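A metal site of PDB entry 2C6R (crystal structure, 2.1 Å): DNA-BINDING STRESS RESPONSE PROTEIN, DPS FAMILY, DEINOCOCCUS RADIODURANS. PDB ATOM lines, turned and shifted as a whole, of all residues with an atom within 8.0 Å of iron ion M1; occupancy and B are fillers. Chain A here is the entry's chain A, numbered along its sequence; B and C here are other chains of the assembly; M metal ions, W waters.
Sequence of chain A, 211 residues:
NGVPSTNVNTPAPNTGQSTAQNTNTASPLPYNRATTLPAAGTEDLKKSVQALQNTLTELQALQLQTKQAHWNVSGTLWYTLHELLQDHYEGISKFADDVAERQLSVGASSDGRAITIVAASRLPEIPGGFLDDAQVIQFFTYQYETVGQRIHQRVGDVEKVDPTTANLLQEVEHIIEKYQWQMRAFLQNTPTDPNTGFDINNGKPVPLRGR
NE1 of Trp 71 of chain B sits close to OD1 of Asp 97 (2.9 Å).
The side-chain amino group of Lys 67 of chain B lies close to the side-chain carboxylate of Asp 97, 2.9 Å away.
O of His 70 of chain B lies within hydrogen-bond range of ND1 of His 82 of chain B (2.7 Å).
Along chain A the residues within 4 Å of iron ion M1 span positions 97 to 101.
Iron ion M1 is bound by OE2 of Glu 101, NE2 of His 70 of chain B, water W2, water W1, OD2 of Asp 97 and OD1 of Asp 97.
Water W2 lies within hydrogen-bond range of OE1 of Gln 86 of chain B (3.0 Å) and NZ of Lys 67 of chain B (3.1 Å).
Water W1 lies within hydrogen-bond range of the side-chain carboxylate (OE1) of Glu 101 (3.3 Å) and a ring nitrogen (NE2) of His 82 of chain B (3.3 Å).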
ATOM      1  N   SER A  93      -2.940  29.338 -22.599  1.00  0.00           N
ATOM      2  CA  SER A  93      -2.713  29.131 -21.153  1.00  0.00           C
ATOM      3  C   SER A  93      -2.530  27.639 -20.792  1.00  0.00           C
ATOM      4  O   SER A  93      -1.673  27.264 -19.993  1.00  0.00           O
ATOM      5  CB  SER A  93      -3.872  29.706 -20.329  1.00  0.00           C
ATOM      6  OG  SER A  93      -3.998  31.117 -20.551  1.00  0.00           O
ATOM      7  N   LYS A  94      -3.356  26.790 -21.405  1.00  0.00           N
ATOM      8  CA  LYS A  94      -3.317  25.348 -21.132  1.00  0.00           C
ATOM      9  C   LYS A  94      -1.952  24.783 -21.561  1.00  0.00           C
ATOM     10  O   LYS A  94      -1.350  24.028 -20.827  1.00  0.00           O
ATOM     11  CB  LYS A  94      -4.461  24.669 -21.902  1.00  0.00           C
ATOM     12  CG  LYS A  94      -4.460  23.118 -21.949  1.00  0.00           C
ATOM     13  CD  LYS A  94      -5.566  22.619 -22.928  1.00  0.00           C
ATOM     14  CE  LYS A  94      -5.103  21.449 -23.810  1.00  0.00           C
ATOM     15  NZ  LYS A  94      -4.128  20.604 -23.060  1.00  0.00           N
ATOM     16  N   ALA A  96       0.852  26.519 -22.019  1.00  0.00           N
ATOM     17  CA  ALA A  96       1.900  27.147 -21.195  1.00  0.00           C
ATOM     18  C   ALA A  96       2.115  26.316 -19.924  1.00  0.00           C
ATOM     19  O   ALA A  96       3.278  26.033 -19.527  1.00  0.00           O
ATOM     20  CB  ALA A  96       1.534  28.590 -20.848  1.00  0.00           C
ATOM     21  N   ASP A  97       1.004  25.924 -19.298  1.00  0.00           N
ATOM     22  CA  ASP A  97       1.071  25.045 -18.139  1.00  0.00           C
ATOM     23  C   ASP A  97       1.693  23.665 -18.461  1.00  0.00           C
ATOM     24  O   ASP A  97       2.503  23.136 -17.669  1.00  0.00           O
ATOM     25  CB  ASP A  97      -0.285  24.931 -17.419  1.00  0.00           C
ATOM     26  CG  ASP A  97      -0.152  24.312 -16.055  1.00  0.00           C
ATOM     27  OD1 ASP A  97       0.273  25.005 -15.106  1.00  0.00           O
ATOM     28  OD2 ASP A  97      -0.443  23.107 -15.930  1.00  0.00           O
ATOM     29  N   ASP A  98       1.341  23.091 -19.607  1.00  0.00           N
ATOM     30  CA  ASP A  98       1.946  21.791 -20.033  1.00  0.00           C
ATOM     31  C   ASP A  98       3.445  21.886 -20.326  1.00  0.00           C
ATOM     32  O   ASP A  98       4.201  20.979 -19.985  1.00  0.00           O
ATOM     33  CB  ASP A  98       1.241  21.239 -21.295  1.00  0.00           C
ATOM     34  CG  ASP A  98      -0.184  20.753 -20.996  1.00  0.00           C
ATOM     35  OD1 ASP A  98      -0.459  20.401 -19.851  1.00  0.00           O
ATOM     36  OD2 ASP A  98      -1.017  20.726 -21.903  1.00  0.00           O
ATOM     37  N   ALA A 100       5.616  24.267 -19.179  1.00  0.00           N
ATOM     38  CA  ALA A 100       6.290  24.468 -17.884  1.00  0.00           C
ATOM     39  C   ALA A 100       6.421  23.180 -17.082  1.00  0.00           C
ATOM     40  O   ALA A 100       7.485  22.893 -16.517  1.00  0.00           O
ATOM     41  CB  ALA A 100       5.587  25.549 -17.083  1.00  0.00           C
ATOM     42  N   GLU A 101       5.363  22.374 -17.046  1.00  0.00           N
ATOM     43  CA  GLU A 101       5.438  21.124 -16.284  1.00  0.00           C
ATOM     44  C   GLU A 101       6.189  20.018 -17.017  1.00  0.00           C
ATOM     45  O   GLU A 101       6.718  19.135 -16.378  1.00  0.00           O
ATOM     46  CB  GLU A 101       4.058  20.696 -15.749  1.00  0.00           C
ATOM     47  CG  GLU A 101       3.525  21.771 -14.744  1.00  0.00           C
ATOM     48  CD  GLU A 101       2.138  21.564 -14.235  1.00  0.00           C
ATOM     49  OE1 GLU A 101       1.488  20.555 -14.609  1.00  0.00           O
ATOM     50  OE2 GLU A 101       1.686  22.417 -13.433  1.00  0.00           O
ATOM     51  N   LYS B  67       1.668  31.237 -10.470  1.00  0.00           N
ATOM     52  CA  LYS B  67       1.981  30.189 -11.441  1.00  0.00           C
ATOM     53  C   LYS B  67       3.441  29.732 -11.273  1.00  0.00           C
ATOM     54  O   LYS B  67       3.726  28.537 -11.289  1.00  0.00           O
ATOM     55  CB  LYS B  67       1.852  30.681 -12.876  1.00  0.00           C
ATOM     56  CG  LYS B  67       0.605  30.286 -13.627  1.00  0.00           C
ATOM     57  CD  LYS B  67       0.235  28.820 -13.536  1.00  0.00           C
ATOM     58  CE  LYS B  67      -1.120  28.673 -14.170  1.00  0.00           C
ATOM     59  NZ  LYS B  67      -1.395  27.271 -14.378  1.00  0.00           N
ATOM     60  N   HIS B  70       3.594  27.690  -8.341  1.00  0.00           N
ATOM     61  CA  HIS B  70       2.836  26.461  -8.686  1.00  0.00           C
ATOM     62  C   HIS B  70       3.770  25.435  -9.350  1.00  0.00           C
ATOM     63  O   HIS B  70       3.802  24.243  -8.955  1.00  0.00           O
ATOM     64  CB  HIS B  70       1.658  26.883  -9.604  1.00  0.00           C
ATOM     65  CG  HIS B  70       0.924  25.761 -10.269  1.00  0.00           C
ATOM     66  ND1 HIS B  70       0.006  24.972  -9.619  1.00  0.00           N
ATOM     67  CD2 HIS B  70       0.911  25.357 -11.564  1.00  0.00           C
ATOM     68  CE1 HIS B  70      -0.514  24.100 -10.453  1.00  0.00           C
ATOM     69  NE2 HIS B  70       0.007  24.326 -11.645  1.00  0.00           N
ATOM     70  N   TRP B  71       4.540  25.896 -10.343  1.00  0.00           N
ATOM     71  CA  TRP B  71       5.503  25.027 -11.040  1.00  0.00           C
ATOM     72  C   TRP B  71       6.720  24.579 -10.218  1.00  0.00           C
ATOM     73  O   TRP B  71       7.112  23.406 -10.282  1.00  0.00           O
ATOM     74  CB  TRP B  71       5.975  25.650 -12.370  1.00  0.00           C
ATOM     75  CG  TRP B  71       4.872  25.984 -13.370  1.00  0.00           C
ATOM     76  CD1 TRP B  71       3.775  25.215 -13.697  1.00  0.00           C
ATOM     77  CD2 TRP B  71       4.792  27.153 -14.200  1.00  0.00           C
ATOM     78  NE1 TRP B  71       3.010  25.854 -14.625  1.00  0.00           N
ATOM     79  CE2 TRP B  71       3.617  27.041 -14.971  1.00  0.00           C
ATOM     80  CE3 TRP B  71       5.630  28.300 -14.365  1.00  0.00           C
ATOM     81  CZ2 TRP B  71       3.217  28.026 -15.913  1.00  0.00           C
ATOM     82  CZ3 TRP B  71       5.224  29.312 -15.280  1.00  0.00           C
ATOM     83  CH2 TRP B  71       4.029  29.160 -16.046  1.00  0.00           C
ATOM     84  N   HIS B  82       1.135  23.495  -4.580  1.00  0.00           N
ATOM     85  CA  HIS B  82       0.841  23.398  -6.001  1.00  0.00           C
ATOM     86  C   HIS B  82      -0.674  23.524  -6.262  1.00  0.00           C
ATOM     87  O   HIS B  82      -1.100  24.286  -7.129  1.00  0.00           O
ATOM     88  CB  HIS B  82       1.429  22.078  -6.527  1.00  0.00           C
ATOM     89  CG  HIS B  82       1.192  21.789  -7.976  1.00  0.00           C
ATOM     90  ND1 HIS B  82       1.890  22.407  -8.997  1.00  0.00           N
ATOM     91  CD2 HIS B  82       0.423  20.833  -8.578  1.00  0.00           C
ATOM     92  CE1 HIS B  82       1.536  21.866 -10.159  1.00  0.00           C
ATOM     93  NE2 HIS B  82       0.652  20.915  -9.927  1.00  0.00           N
ATOM     94  N   GLU B  83      -1.467  22.780  -5.490  1.00  0.00           N
ATOM     95  CA  GLU B  83      -2.948  22.809  -5.602  1.00  0.00           C
ATOM     96  C   GLU B  83      -3.537  24.128  -5.076  1.00  0.00           C
ATOM     97  O   GLU B  83      -4.380  24.760  -5.743  1.00  0.00           O
ATOM     98  CB  GLU B  83      -3.574  21.634  -4.812  1.00  0.00           C
ATOM     99  CG  GLU B  83      -3.226  20.217  -5.336  1.00  0.00           C
ATOM    100  CD  GLU B  83      -3.628  20.044  -6.783  1.00  0.00           C
ATOM    101  OE1 GLU B  83      -4.841  20.038  -7.076  1.00  0.00           O
ATOM    102  OE2 GLU B  83      -2.743  19.936  -7.667  1.00  0.00           O
ATOM    103  N   GLN B  86      -2.810  26.946  -7.451  1.00  0.00           N
ATOM    104  CA  GLN B  86      -3.682  26.880  -8.648  1.00  0.00           C
ATOM    105  C   GLN B  86      -5.044  27.543  -8.377  1.00  0.00           C
ATOM    106  O   GLN B  86      -5.552  28.300  -9.207  1.00  0.00           O
ATOM    107  CB  GLN B  86      -3.814  25.447  -9.177  1.00  0.00           C
ATOM    108  CG  GLN B  86      -4.657  25.270 -10.466  1.00  0.00           C
ATOM    109  CD  GLN B  86      -4.190  26.143 -11.623  1.00  0.00           C
ATOM    110  OE1 GLN B  86      -2.982  26.379 -11.813  1.00  0.00           O
ATOM    111  NE2 GLN B  86      -5.142  26.610 -12.423  1.00  0.00           N
ATOM    112  N   LYS C 178       5.897  12.941 -15.752  1.00  0.00           N
ATOM    113  CA  LYS C 178       5.209  13.969 -14.952  1.00  0.00           C
ATOM    114  C   LYS C 178       4.981  13.482 -13.519  1.00  0.00           C
ATOM    115  O   LYS C 178       5.230  14.208 -12.555  1.00  0.00           O
ATOM    116  CB  LYS C 178       3.879  14.364 -15.611  1.00  0.00           C
ATOM    117  CG  LYS C 178       3.032  15.371 -14.807  1.00  0.00           C
ATOM    118  CD  LYS C 178       1.855  15.780 -15.661  1.00  0.00           C
ATOM    119  CE  LYS C 178       0.902  16.657 -14.903  1.00  0.00           C
ATOM    120  NZ  LYS C 178      -0.190  16.997 -15.853  1.00  0.00           N
ATOM    121  N   TRP C 181       8.249  13.601 -11.531  1.00  0.00           N
ATOM    122  CA  TRP C 181       8.475  14.930 -10.989  1.00  0.00           C
ATOM    123  C   TRP C 181       7.598  15.157  -9.738  1.00  0.00           C
ATOM    124  O   TRP C 181       8.054  15.682  -8.730  1.00  0.00           O
ATOM    125  CB  TRP C 181       8.225  16.002 -12.078  1.00  0.00           C
ATOM    126  CG  TRP C 181       7.726  17.327 -11.487  1.00  0.00           C
ATOM    127  CD1 TRP C 181       8.365  18.116 -10.581  1.00  0.00           C
ATOM    128  CD2 TRP C 181       6.491  17.973 -11.784  1.00  0.00           C
ATOM    129  NE1 TRP C 181       7.597  19.224 -10.275  1.00  0.00           N
ATOM    130  CE2 TRP C 181       6.449  19.176 -11.025  1.00  0.00           C
ATOM    131  CE3 TRP C 181       5.431  17.687 -12.652  1.00  0.00           C
ATOM    132  CZ2 TRP C 181       5.361  20.063 -11.078  1.00  0.00           C
ATOM    133  CZ3 TRP C 181       4.333  18.571 -12.685  1.00  0.00           C
ATOM    134  CH2 TRP C 181       4.338  19.747 -11.919  1.00  0.00           C
ATOM    135  N   GLN C 182       6.331  14.745  -9.807  1.00  0.00           N
ATOM    136  CA  GLN C 182       5.417  14.993  -8.693  1.00  0.00           C
ATOM    137  C   GLN C 182       5.864  14.255  -7.413  1.00  0.00           C
ATOM    138  O   GLN C 182       5.576  14.705  -6.315  1.00  0.00           O
ATOM    139  CB  GLN C 182       3.951  14.666  -9.092  1.00  0.00           C
ATOM    140  CG  GLN C 182       3.400  15.605 -10.187  1.00  0.00           C
ATOM    141  CD  GLN C 182       1.949  15.361 -10.547  1.00  0.00           C
ATOM    142  OE1 GLN C 182       1.425  14.245 -10.420  1.00  0.00           O
ATOM    143  NE2 GLN C 182       1.270  16.420 -11.010  1.00  0.00           N
HETATM  144 FE    FE M   1      -0.224  23.248 -13.576  1.00  0.00          FE
HETATM  145 FE    FE M   2      -2.473  20.514 -18.587  1.00  0.00          FE
HETATM  146  O   HOH W   1      -1.125  21.302 -12.740  1.00  0.00           O
HETATM  147  O   HOH W   2      -2.200  24.308 -13.790  1.00  0.00           O
